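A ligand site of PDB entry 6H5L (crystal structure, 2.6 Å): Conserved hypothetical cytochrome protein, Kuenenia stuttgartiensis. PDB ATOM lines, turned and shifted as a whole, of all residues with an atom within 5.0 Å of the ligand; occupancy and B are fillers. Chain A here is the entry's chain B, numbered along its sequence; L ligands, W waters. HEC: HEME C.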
ATOM      1  N   LYS A  50     -16.897   3.115  -4.301  1.00  0.00           N
ATOM      2  CA  LYS A  50     -17.793   2.018  -4.685  1.00  0.00           C
ATOM      3  C   LYS A  50     -18.229   1.206  -3.465  1.00  0.00           C
ATOM      4  O   LYS A  50     -19.371   0.735  -3.417  1.00  0.00           O
ATOM      5  CB  LYS A  50     -17.115   1.113  -5.704  1.00  0.00           C
ATOM      6  CG  LYS A  50     -16.926   1.707  -7.085  1.00  0.00           C
ATOM      7  CD  LYS A  50     -16.411   0.645  -8.045  1.00  0.00           C
ATOM      8  CE  LYS A  50     -16.075   1.211  -9.415  1.00  0.00           C
ATOM      9  NZ  LYS A  50     -15.533   0.147 -10.316  1.00  0.00           N
ATOM     10  N   PHE A  51     -17.336   1.017  -2.503  1.00  0.00           N
ATOM     11  CA  PHE A  51     -17.495   0.004  -1.469  1.00  0.00           C
ATOM     12  C   PHE A  51     -17.567   0.671  -0.102  1.00  0.00           C
ATOM     13  O   PHE A  51     -16.548   1.134   0.434  1.00  0.00           O
ATOM     14  CB  PHE A  51     -16.349  -1.005  -1.564  1.00  0.00           C
ATOM     15  CG  PHE A  51     -16.051  -1.415  -2.977  1.00  0.00           C
ATOM     16  CD1 PHE A  51     -16.996  -2.094  -3.723  1.00  0.00           C
ATOM     17  CD2 PHE A  51     -14.827  -1.102  -3.557  1.00  0.00           C
ATOM     18  CE1 PHE A  51     -16.727  -2.466  -5.027  1.00  0.00           C
ATOM     19  CE2 PHE A  51     -14.558  -1.474  -4.861  1.00  0.00           C
ATOM     20  CZ  PHE A  51     -15.502  -2.160  -5.594  1.00  0.00           C
ATOM     21  N   TYR A 132     -34.012 -11.361  -9.830  1.00  0.00           N
ATOM     22  CA  TYR A 132     -32.902 -11.089 -10.745  1.00  0.00           C
ATOM     23  C   TYR A 132     -33.366 -11.028 -12.190  1.00  0.00           C
ATOM     24  O   TYR A 132     -32.841 -10.239 -12.990  1.00  0.00           O
ATOM     25  CB  TYR A 132     -31.825 -12.168 -10.570  1.00  0.00           C
ATOM     26  CG  TYR A 132     -30.607 -12.029 -11.455  1.00  0.00           C
ATOM     27  CD1 TYR A 132     -30.596 -12.540 -12.747  1.00  0.00           C
ATOM     28  CD2 TYR A 132     -29.463 -11.396 -10.998  1.00  0.00           C
ATOM     29  CE1 TYR A 132     -29.490 -12.423 -13.561  1.00  0.00           C
ATOM     30  CE2 TYR A 132     -28.333 -11.279 -11.809  1.00  0.00           C
ATOM     31  CZ  TYR A 132     -28.361 -11.796 -13.090  1.00  0.00           C
ATOM     32  OH  TYR A 132     -27.255 -11.679 -13.904  1.00  0.00           O
ATOM     33  N   LEU A 136     -36.536  -7.054 -11.412  1.00  0.00           N
ATOM     34  CA  LEU A 136     -35.573  -5.979 -11.627  1.00  0.00           C
ATOM     35  C   LEU A 136     -34.717  -6.151 -12.875  1.00  0.00           C
ATOM     36  O   LEU A 136     -33.977  -5.227 -13.224  1.00  0.00           O
ATOM     37  CB  LEU A 136     -34.660  -5.827 -10.401  1.00  0.00           C
ATOM     38  CG  LEU A 136     -35.393  -5.466  -9.104  1.00  0.00           C
ATOM     39  CD1 LEU A 136     -34.437  -5.376  -7.930  1.00  0.00           C
ATOM     40  CD2 LEU A 136     -36.166  -4.162  -9.273  1.00  0.00           C
ATOM     41  N   GLU A 137     -34.782  -7.306 -13.538  1.00  0.00           N
ATOM     42  CA  GLU A 137     -34.115  -7.544 -14.821  1.00  0.00           C
ATOM     43  C   GLU A 137     -32.636  -7.179 -14.758  1.00  0.00           C
ATOM     44  O   GLU A 137     -32.129  -6.329 -15.503  1.00  0.00           O
ATOM     45  CB  GLU A 137     -34.824  -6.788 -15.951  1.00  0.00           C
ATOM     46  CG  GLU A 137     -36.295  -7.146 -16.107  1.00  0.00           C
ATOM     47  CD  GLU A 137     -36.960  -6.391 -17.252  1.00  0.00           C
ATOM     48  OE1 GLU A 137     -37.424  -7.042 -18.207  1.00  0.00           O
ATOM     49  OE2 GLU A 137     -37.000  -5.137 -17.182  1.00  0.00           O
ATOM     50  N   CYS A 138     -31.931  -7.862 -13.854  1.00  0.00           N
ATOM     51  CA  CYS A 138     -30.502  -7.640 -13.717  1.00  0.00           C
ATOM     52  C   CYS A 138     -29.720  -8.205 -14.905  1.00  0.00           C
ATOM     53  O   CYS A 138     -28.579  -7.791 -15.132  1.00  0.00           O
ATOM     54  CB  CYS A 138     -29.990  -8.267 -12.417  1.00  0.00           C
ATOM     55  SG  CYS A 138     -31.113  -8.052 -11.021  1.00  0.00           S
ATOM     56  N   LYS A 140     -30.070  -7.463 -17.805  1.00  0.00           N
ATOM     57  CA  LYS A 140     -29.830  -6.371 -18.742  1.00  0.00           C
ATOM     58  C   LYS A 140     -28.342  -6.041 -18.839  1.00  0.00           C
ATOM     59  O   LYS A 140     -27.745  -6.079 -19.928  1.00  0.00           O
ATOM     60  CB  LYS A 140     -30.641  -5.133 -18.334  1.00  0.00           C
ATOM     61  CG  LYS A 140     -32.129  -5.233 -18.633  1.00  0.00           C
ATOM     62  CD  LYS A 140     -32.386  -5.157 -20.141  1.00  0.00           C
ATOM     63  CE  LYS A 140     -33.870  -5.292 -20.442  1.00  0.00           C
ATOM     64  NZ  LYS A 140     -34.666  -4.213 -19.812  1.00  0.00           N
ATOM     65  N   CYS A 141     -27.721  -5.725 -17.704  1.00  0.00           N
ATOM     66  CA  CYS A 141     -26.294  -5.433 -17.668  1.00  0.00           C
ATOM     67  C   CYS A 141     -25.445  -6.692 -17.466  1.00  0.00           C
ATOM     68  O   CYS A 141     -24.398  -6.837 -18.105  1.00  0.00           O
ATOM     69  CB  CYS A 141     -25.984  -4.434 -16.547  1.00  0.00           C
ATOM     70  SG  CYS A 141     -26.775  -2.805 -16.722  1.00  0.00           S
ATOM     71  N   HIS A 142     -25.893  -7.612 -16.605  1.00  0.00           N
ATOM     72  CA  HIS A 142     -25.059  -8.725 -16.189  1.00  0.00           C
ATOM     73  C   HIS A 142     -25.269 -10.009 -16.979  1.00  0.00           C
ATOM     74  O   HIS A 142     -24.420 -10.898 -16.932  1.00  0.00           O
ATOM     75  CB  HIS A 142     -25.282  -9.019 -14.697  1.00  0.00           C
ATOM     76  CG  HIS A 142     -24.759  -7.954 -13.790  1.00  0.00           C
ATOM     77  ND1 HIS A 142     -23.419  -7.845 -13.472  1.00  0.00           N
ATOM     78  CD2 HIS A 142     -25.387  -6.958 -13.122  1.00  0.00           C
ATOM     79  CE1 HIS A 142     -23.250  -6.820 -12.649  1.00  0.00           C
ATOM     80  NE2 HIS A 142     -24.432  -6.269 -12.429  1.00  0.00           N
ATOM     81  N   GLN A 156     -22.294   0.645 -20.727  1.00  0.00           N
ATOM     82  CA  GLN A 156     -22.293   1.271 -19.413  1.00  0.00           C
ATOM     83  C   GLN A 156     -21.043   2.136 -19.233  1.00  0.00           C
ATOM     84  O   GLN A 156     -19.987   1.862 -19.801  1.00  0.00           O
ATOM     85  CB  GLN A 156     -22.351   0.198 -18.321  1.00  0.00           C
ATOM     86  CG  GLN A 156     -23.549  -0.718 -18.422  1.00  0.00           C
ATOM     87  CD  GLN A 156     -24.865   0.038 -18.407  1.00  0.00           C
ATOM     88  OE1 GLN A 156     -25.052   0.956 -17.606  1.00  0.00           O
ATOM     89  NE2 GLN A 156     -25.780  -0.342 -19.291  1.00  0.00           N
ATOM     90  N   ILE A 164     -17.544   1.199 -18.009  1.00  0.00           N
ATOM     91  CA  ILE A 164     -17.554   0.217 -16.928  1.00  0.00           C
ATOM     92  C   ILE A 164     -18.489  -0.913 -17.369  1.00  0.00           C
ATOM     93  O   ILE A 164     -19.688  -0.923 -17.075  1.00  0.00           O
ATOM     94  CB  ILE A 164     -17.975   0.821 -15.577  1.00  0.00           C
ATOM     95  CG1 ILE A 164     -18.020  -0.245 -14.483  1.00  0.00           C
ATOM     96  CG2 ILE A 164     -19.293   1.594 -15.688  1.00  0.00           C
ATOM     97  CD1 ILE A 164     -17.982   0.339 -13.076  1.00  0.00           C
ATOM     98  N   LYS A 165     -17.928  -1.884 -18.086  1.00  0.00           N
ATOM     99  CA  LYS A 165     -18.675  -3.061 -18.483  1.00  0.00           C
ATOM    100  C   LYS A 165     -18.649  -4.075 -17.351  1.00  0.00           C
ATOM    101  O   LYS A 165     -17.563  -4.458 -16.914  1.00  0.00           O
ATOM    102  CB  LYS A 165     -18.076  -3.666 -19.742  1.00  0.00           C
ATOM    103  CG  LYS A 165     -18.796  -4.870 -20.291  1.00  0.00           C
ATOM    104  CD  LYS A 165     -18.226  -5.277 -21.648  1.00  0.00           C
ATOM    105  CE  LYS A 165     -18.848  -6.571 -22.160  1.00  0.00           C
ATOM    106  NZ  LYS A 165     -18.490  -7.769 -21.340  1.00  0.00           N
ATOM    107  N   PRO A 166     -19.800  -4.484 -16.820  1.00  0.00           N
ATOM    108  CA  PRO A 166     -19.800  -5.343 -15.617  1.00  0.00           C
ATOM    109  C   PRO A 166     -19.002  -6.616 -15.842  1.00  0.00           C
ATOM    110  O   PRO A 166     -19.289  -7.411 -16.735  1.00  0.00           O
ATOM    111  CB  PRO A 166     -21.284  -5.626 -15.388  1.00  0.00           C
ATOM    112  CG  PRO A 166     -21.936  -5.384 -16.717  1.00  0.00           C
ATOM    113  CD  PRO A 166     -21.162  -4.271 -17.352  1.00  0.00           C
ATOM    114  N   PHE A 167     -17.973  -6.795 -15.014  1.00  0.00           N
ATOM    115  CA  PHE A 167     -17.108  -7.953 -15.130  1.00  0.00           C
ATOM    116  C   PHE A 167     -17.899  -9.232 -14.873  1.00  0.00           C
ATOM    117  O   PHE A 167     -18.924  -9.247 -14.188  1.00  0.00           O
ATOM    118  CB  PHE A 167     -15.933  -7.852 -14.158  1.00  0.00           C
ATOM    119  CG  PHE A 167     -16.333  -7.893 -12.709  1.00  0.00           C
ATOM    120  CD1 PHE A 167     -16.665  -6.728 -12.037  1.00  0.00           C
ATOM    121  CD2 PHE A 167     -16.382  -9.099 -12.022  1.00  0.00           C
ATOM    122  CE1 PHE A 167     -17.036  -6.765 -10.700  1.00  0.00           C
ATOM    123  CE2 PHE A 167     -16.761  -9.136 -10.692  1.00  0.00           C
ATOM    124  CZ  PHE A 167     -17.082  -7.972 -10.030  1.00  0.00           C
ATOM    125  N   PHE A 169     -18.791 -12.081 -12.925  1.00  0.00           N
ATOM    126  CA  PHE A 169     -18.664 -12.418 -11.507  1.00  0.00           C
ATOM    127  C   PHE A 169     -18.916 -13.890 -11.218  1.00  0.00           C
ATOM    128  O   PHE A 169     -18.911 -14.275 -10.042  1.00  0.00           O
ATOM    129  CB  PHE A 169     -19.586 -11.540 -10.654  1.00  0.00           C
ATOM    130  CG  PHE A 169     -21.061 -11.709 -10.932  1.00  0.00           C
ATOM    131  CD1 PHE A 169     -21.750 -12.839 -10.493  1.00  0.00           C
ATOM    132  CD2 PHE A 169     -21.770 -10.715 -11.575  1.00  0.00           C
ATOM    133  CE1 PHE A 169     -23.095 -12.985 -10.732  1.00  0.00           C
ATOM    134  CE2 PHE A 169     -23.132 -10.846 -11.813  1.00  0.00           C
ATOM    135  CZ  PHE A 169     -23.794 -11.991 -11.385  1.00  0.00           C
ATOM    136  N   PHE A 174     -15.621 -11.038  -6.402  1.00  0.00           N
ATOM    137  CA  PHE A 174     -16.304  -9.758  -6.334  1.00  0.00           C
ATOM    138  C   PHE A 174     -15.351  -8.681  -5.850  1.00  0.00           C
ATOM    139  O   PHE A 174     -14.455  -8.925  -5.041  1.00  0.00           O
ATOM    140  CB  PHE A 174     -17.521  -9.851  -5.412  1.00  0.00           C
ATOM    141  CG  PHE A 174     -18.497 -10.925  -5.789  1.00  0.00           C
ATOM    142  CD1 PHE A 174     -19.473 -10.699  -6.729  1.00  0.00           C
ATOM    143  CD2 PHE A 174     -18.411 -12.183  -5.203  1.00  0.00           C
ATOM    144  CE1 PHE A 174     -20.373 -11.700  -7.074  1.00  0.00           C
ATOM    145  CE2 PHE A 174     -19.304 -13.184  -5.541  1.00  0.00           C
ATOM    146  CZ  PHE A 174     -20.292 -12.936  -6.484  1.00  0.00           C
ATOM    147  N   LYS A 175     -15.550  -7.459  -6.366  1.00  0.00           N
ATOM    148  CA  LYS A 175     -14.616  -6.377  -6.074  1.00  0.00           C
ATOM    149  C   LYS A 175     -14.690  -5.951  -4.615  1.00  0.00           C
ATOM    150  O   LYS A 175     -13.662  -5.603  -4.009  1.00  0.00           O
ATOM    151  CB  LYS A 175     -14.893  -5.196  -7.001  1.00  0.00           C
ATOM    152  CG  LYS A 175     -14.551  -5.460  -8.453  1.00  0.00           C
ATOM    153  CD  LYS A 175     -14.435  -4.164  -9.241  1.00  0.00           C
ATOM    154  CE  LYS A 175     -14.022  -4.428 -10.681  1.00  0.00           C
ATOM    155  NZ  LYS A 175     -13.731  -3.162 -11.399  1.00  0.00           N
ATOM    156  N   GLY A 176     -15.876  -5.965  -4.024  1.00  0.00           N
ATOM    157  CA  GLY A 176     -16.050  -5.608  -2.631  1.00  0.00           C
ATOM    158  C   GLY A 176     -15.860  -6.726  -1.637  1.00  0.00           C
ATOM    159  O   GLY A 176     -15.925  -6.484  -0.427  1.00  0.00           O
ATOM    160  N   GLY A 177     -15.637  -7.951  -2.100  1.00  0.00           N
ATOM    161  CA  GLY A 177     -15.511  -9.101  -1.239  1.00  0.00           C
ATOM    162  C   GLY A 177     -16.493 -10.186  -1.651  1.00  0.00           C
ATOM    163  O   GLY A 177     -17.592  -9.898  -2.123  1.00  0.00           O
ATOM    164  N   VAL A 183     -21.747  -9.234  -0.436  1.00  0.00           N
ATOM    165  CA  VAL A 183     -22.651  -9.073  -1.568  1.00  0.00           C
ATOM    166  C   VAL A 183     -23.958  -8.445  -1.118  1.00  0.00           C
ATOM    167  O   VAL A 183     -24.539  -7.612  -1.818  1.00  0.00           O
ATOM    168  CB  VAL A 183     -22.872 -10.428  -2.272  1.00  0.00           C
ATOM    169  CG1 VAL A 183     -23.915 -10.305  -3.363  1.00  0.00           C
ATOM    170  CG2 VAL A 183     -21.559 -10.939  -2.849  1.00  0.00           C
ATOM    171  N   ARG A 186     -23.475  -4.703  -0.866  1.00  0.00           N
ATOM    172  CA  ARG A 186     -23.496  -3.999  -2.148  1.00  0.00           C
ATOM    173  C   ARG A 186     -24.927  -3.692  -2.577  1.00  0.00           C
ATOM    174  O   ARG A 186     -25.215  -2.580  -3.052  1.00  0.00           O
ATOM    175  CB  ARG A 186     -22.783  -4.824  -3.221  1.00  0.00           C
ATOM    176  CG  ARG A 186     -21.357  -5.217  -2.880  1.00  0.00           C
ATOM    177  CD  ARG A 186     -20.401  -4.023  -2.870  1.00  0.00           C
ATOM    178  NE  ARG A 186     -20.370  -3.329  -1.592  1.00  0.00           N
ATOM    179  CZ  ARG A 186     -19.634  -3.717  -0.559  1.00  0.00           C
ATOM    180  NH1 ARG A 186     -18.862  -4.793  -0.646  1.00  0.00           N
ATOM    181  NH2 ARG A 186     -19.667  -3.020   0.572  1.00  0.00           N
ATOM    182  N   PHE A 187     -25.834  -4.652  -2.426  1.00  0.00           N
ATOM    183  CA  PHE A 187     -27.224  -4.440  -2.804  1.00  0.00           C
ATOM    184  C   PHE A 187     -27.936  -3.491  -1.854  1.00  0.00           C
ATOM    185  O   PHE A 187     -28.938  -2.870  -2.236  1.00  0.00           O
ATOM    186  CB  PHE A 187     -27.979  -5.767  -2.860  1.00  0.00           C
ATOM    187  CG  PHE A 187     -27.364  -6.777  -3.794  1.00  0.00           C
ATOM    188  CD1 PHE A 187     -26.533  -6.385  -4.823  1.00  0.00           C
ATOM    189  CD2 PHE A 187     -27.628  -8.131  -3.628  1.00  0.00           C
ATOM    190  CE1 PHE A 187     -25.970  -7.312  -5.685  1.00  0.00           C
ATOM    191  CE2 PHE A 187     -27.070  -9.064  -4.485  1.00  0.00           C
ATOM    192  CZ  PHE A 187     -26.239  -8.658  -5.515  1.00  0.00           C
ATOM    193  N   LEU A 191     -23.284   1.164  -5.416  1.00  0.00           N
ATOM    194  CA  LEU A 191     -21.897   1.473  -5.777  1.00  0.00           C
ATOM    195  C   LEU A 191     -21.856   2.896  -6.319  1.00  0.00           C
ATOM    196  O   LEU A 191     -22.212   3.144  -7.477  1.00  0.00           O
ATOM    197  CB  LEU A 191     -21.372   0.449  -6.791  1.00  0.00           C
ATOM    198  CG  LEU A 191     -20.882  -0.885  -6.231  1.00  0.00           C
ATOM    199  CD1 LEU A 191     -22.027  -1.732  -5.674  1.00  0.00           C
ATOM    200  CD2 LEU A 191     -20.107  -1.665  -7.284  1.00  0.00           C
ATOM    201  N   THR A 194     -21.124   4.521 -10.209  1.00  0.00           N
ATOM    202  CA  THR A 194     -21.402   3.530 -11.236  1.00  0.00           C
ATOM    203  C   THR A 194     -22.896   3.422 -11.459  1.00  0.00           C
ATOM    204  O   THR A 194     -23.690   3.784 -10.580  1.00  0.00           O
ATOM    205  CB  THR A 194     -20.823   2.154 -10.844  1.00  0.00           C
ATOM    206  OG1 THR A 194     -21.634   1.585  -9.808  1.00  0.00           O
ATOM    207  CG2 THR A 194     -19.401   2.292 -10.343  1.00  0.00           C
ATOM    208  N   PRO A 195     -23.322   2.924 -12.631  1.00  0.00           N
ATOM    209  CA  PRO A 195     -24.760   2.709 -12.859  1.00  0.00           C
ATOM    210  C   PRO A 195     -25.361   1.591 -12.015  1.00  0.00           C
ATOM    211  O   PRO A 195     -26.563   1.318 -12.147  1.00  0.00           O
ATOM    212  CB  PRO A 195     -24.832   2.372 -14.363  1.00  0.00           C
ATOM    213  CG  PRO A 195     -23.486   1.847 -14.691  1.00  0.00           C
ATOM    214  CD  PRO A 195     -22.532   2.642 -13.836  1.00  0.00           C
ATOM    215  N   MET A 196     -24.572   0.932 -11.168  1.00  0.00           N
ATOM    216  CA  MET A 196     -25.069  -0.074 -10.238  1.00  0.00           C
ATOM    217  C   MET A 196     -25.654   0.627  -9.014  1.00  0.00           C
ATOM    218  O   MET A 196     -24.910   1.105  -8.152  1.00  0.00           O
ATOM    219  CB  MET A 196     -23.945  -1.033  -9.822  1.00  0.00           C
ATOM    220  CG  MET A 196     -24.352  -2.074  -8.797  1.00  0.00           C
ATOM    221  SD  MET A 196     -25.441  -3.341  -9.455  1.00  0.00           S
ATOM    222  CE  MET A 196     -25.906  -4.185  -7.938  1.00  0.00           C
ATOM    223  N   PHE A 199     -30.381  -1.027  -3.920  1.00  0.00           N
ATOM    224  CA  PHE A 199     -31.705  -1.634  -3.894  1.00  0.00           C
ATOM    225  C   PHE A 199     -32.262  -1.697  -2.471  1.00  0.00           C
ATOM    226  O   PHE A 199     -33.133  -2.526  -2.183  1.00  0.00           O
ATOM    227  CB  PHE A 199     -31.653  -3.020  -4.527  1.00  0.00           C
ATOM    228  CG  PHE A 199     -31.202  -2.999  -5.954  1.00  0.00           C
ATOM    229  CD1 PHE A 199     -32.100  -2.787  -6.984  1.00  0.00           C
ATOM    230  CD2 PHE A 199     -29.865  -3.176  -6.272  1.00  0.00           C
ATOM    231  CE1 PHE A 199     -31.683  -2.749  -8.295  1.00  0.00           C
ATOM    232  CE2 PHE A 199     -29.436  -3.145  -7.580  1.00  0.00           C
ATOM    233  CZ  PHE A 199     -30.348  -2.925  -8.596  1.00  0.00           C
ATOM    234  N   LEU A 211     -31.920 -12.408  -3.018  1.00  0.00           N
ATOM    235  CA  LEU A 211     -31.153 -12.028  -4.193  1.00  0.00           C
ATOM    236  C   LEU A 211     -29.685 -12.408  -4.034  1.00  0.00           C
ATOM    237  O   LEU A 211     -29.056 -12.895  -4.980  1.00  0.00           O
ATOM    238  CB  LEU A 211     -31.305 -10.537  -4.452  1.00  0.00           C
ATOM    239  CG  LEU A 211     -30.578  -9.917  -5.649  1.00  0.00           C
ATOM    240  CD1 LEU A 211     -31.120 -10.483  -6.955  1.00  0.00           C
ATOM    241  CD2 LEU A 211     -30.722  -8.409  -5.607  1.00  0.00           C
ATOM    242  N   VAL A 215     -27.383 -14.865  -6.446  1.00  0.00           N
ATOM    243  CA  VAL A 215     -26.141 -14.383  -7.043  1.00  0.00           C
ATOM    244  C   VAL A 215     -24.990 -15.315  -6.713  1.00  0.00           C
ATOM    245  O   VAL A 215     -24.165 -15.648  -7.583  1.00  0.00           O
ATOM    246  CB  VAL A 215     -25.846 -12.943  -6.586  1.00  0.00           C
ATOM    247  CG1 VAL A 215     -24.453 -12.514  -7.033  1.00  0.00           C
ATOM    248  CG2 VAL A 215     -26.894 -11.982  -7.146  1.00  0.00           C
HETATM  249 FE   HEC L   1     -24.955  -4.838 -11.125  1.00  0.00          FE
HETATM  250  CHA HEC L   1     -21.735  -4.502  -9.976  1.00  0.00           C
HETATM  251  CHB HEC L   1     -25.407  -7.536  -9.044  1.00  0.00           C
HETATM  252  CHC HEC L   1     -28.272  -4.973 -11.997  1.00  0.00           C
HETATM  253  CHD HEC L   1     -24.344  -2.686 -13.714  1.00  0.00           C
HETATM  254  NA  HEC L   1     -23.796  -5.801  -9.719  1.00  0.00           N
HETATM  255  C1A HEC L   1     -22.457  -5.571  -9.494  1.00  0.00           C
HETATM  256  C2A HEC L   1     -21.946  -6.640  -8.651  1.00  0.00           C
HETATM  257  C3A HEC L   1     -22.964  -7.479  -8.402  1.00  0.00           C
HETATM  258  C4A HEC L   1     -24.142  -6.972  -9.066  1.00  0.00           C
HETATM  259  CMA HEC L   1     -22.893  -8.770  -7.544  1.00  0.00           C
HETATM  260  CAA HEC L   1     -20.495  -6.787  -8.156  1.00  0.00           C
HETATM  261  CBA HEC L   1     -20.387  -6.375  -6.693  1.00  0.00           C
HETATM  262  CGA HEC L   1     -18.954  -6.482  -6.239  1.00  0.00           C
HETATM  263  O1A HEC L   1     -18.067  -6.729  -7.093  1.00  0.00           O
HETATM  264  O2A HEC L   1     -18.697  -6.312  -5.017  1.00  0.00           O
HETATM  265  NB  HEC L   1     -26.533  -6.088 -10.672  1.00  0.00           N
HETATM  266  C1B HEC L   1     -26.519  -7.026  -9.661  1.00  0.00           C
HETATM  267  C2B HEC L   1     -27.891  -7.375  -9.352  1.00  0.00           C
HETATM  268  C3B HEC L   1     -28.693  -6.671 -10.176  1.00  0.00           C
HETATM  269  C4B HEC L   1     -27.846  -5.845 -11.015  1.00  0.00           C
HETATM  270  CMB HEC L   1     -28.302  -8.405  -8.281  1.00  0.00           C
HETATM  271  CAB HEC L   1     -30.242  -6.694 -10.239  1.00  0.00           C
HETATM  272  CBB HEC L   1     -30.905  -6.262  -8.919  1.00  0.00           C
HETATM  273  NC  HEC L   1     -26.089  -4.024 -12.613  1.00  0.00           N
HETATM  274  C1C HEC L   1     -27.463  -4.146 -12.742  1.00  0.00           C
HETATM  275  C2C HEC L   1     -27.917  -3.150 -13.692  1.00  0.00           C
HETATM  276  C3C HEC L   1     -26.817  -2.616 -14.266  1.00  0.00           C
HETATM  277  C4C HEC L   1     -25.661  -3.087 -13.527  1.00  0.00           C
HETATM  278  CMC HEC L   1     -29.355  -3.080 -14.249  1.00  0.00           C
HETATM  279  CAC HEC L   1     -26.797  -1.567 -15.404  1.00  0.00           C
HETATM  280  CBC HEC L   1     -27.394  -0.232 -14.919  1.00  0.00           C
HETATM  281  ND  HEC L   1     -23.287  -3.767 -11.764  1.00  0.00           N
HETATM  282  C1D HEC L   1     -23.292  -2.898 -12.850  1.00  0.00           C
HETATM  283  C2D HEC L   1     -21.998  -2.246 -12.922  1.00  0.00           C
HETATM  284  C3D HEC L   1     -21.185  -2.822 -11.753  1.00  0.00           C
HETATM  285  C4D HEC L   1     -22.062  -3.754 -11.087  1.00  0.00           C
HETATM  286  CMD HEC L   1     -21.547  -1.207 -13.963  1.00  0.00           C
HETATM  287  CAD HEC L   1     -19.723  -2.473 -11.362  1.00  0.00           C
HETATM  288  CBD HEC L   1     -18.760  -3.281 -12.220  1.00  0.00           C
HETATM  289  CGD HEC L   1     -17.339  -2.850 -11.949  1.00  0.00           C
HETATM  290  O1D HEC L   1     -17.121  -2.082 -10.973  1.00  0.00           O
HETATM  291  O2D HEC L   1     -16.429  -3.267 -12.714  1.00  0.00           O
HETATM  292  O   HOH W   1     -18.991  -7.279  -2.057  1.00  0.00           O
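The backbone NH of Gly 176 sits at hydrogen-bond distance from an oxygen (O2A) of the ligand, 3.0 Å away.
An iron atom (FE) of the ligand is bound by a ring nitrogen (NE2) of His 142, 2.0 Å away.
The backbone NH of Lys 175 sits at hydrogen-bond distance from an oxygen (O1A) of the ligand (2.7 Å).
An oxygen (O1D) of the ligand lies within salt-bridge range of the side-chain amino group (NZ) of Lys 50 (2.8 Å).
The side-chain sulfur of Cys 141 is bonded to a carbon (CAC) of the ligand (1.8 Å).
NZ of Lys 175 is in salt-bridge range of O2D of the ligand (3.0 Å).
The side-chain sulfur (SD) of Met 196 is bound to an iron atom (FE) of the ligand.
The side-chain sulfur of Cys 138 is covalently linked to a carbon (CAB) of the ligand (1.8 Å).
N of Phe 199 is in hydrogen-bond range of O of Phe 187 (2.9 Å).
O of Tyr 132 lies within hydrogen-bond range of N of Cys 138 (2.7 Å).
N of Ile 164 sits at hydrogen-bond distance from O of Gln 156 (3.1 Å).
NE2 of Gln 156 sits at hydrogen-bond distance from SG of Cys 141 (3.7 Å).
OG1 of Thr 194 sits close to N of Met 196, 3.3 Å away.
O of Gly 176 is in hydrogen-bond range of NH1 of Arg 186.
The backbone carbonyl oxygen (O) of Met 196 is in hydrogen-bond range of the backbone NH (N) of Leu 191 (3.2 Å).
Leu 136 touches the ligand.
Gln 156 touches the ligand (OE1 to CBC, 3.8 Å).
CD1 of Ile 164 touches O1D of the ligand (3.3 Å).
Phe 167 touches the ligand.
Phe 174 touches the ligand (C to O1A, 3.6 Å).
CD of Arg 186 touches O2A of the ligand (3.6 Å).
Phe 187 touches the ligand (CE1 to CHB, 3.4 Å).
Pro 195 touches the ligand (O to CBC, 3.3 Å).
Phe 199 touches the ligand (CZ to CBB, 3.4 Å).
Leu 211 touches the ligand.
The nearest printed residue that does not touch the ligand is Val 215 (4.01 Å).
Water W1 lies within hydrogen-bond range of the guanidinium group of Arg 186 (2.9 Å), the backbone carbonyl oxygen of Gly 177 (3.0 Å) and an oxygen (O2A) of the ligand (3.1 Å).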
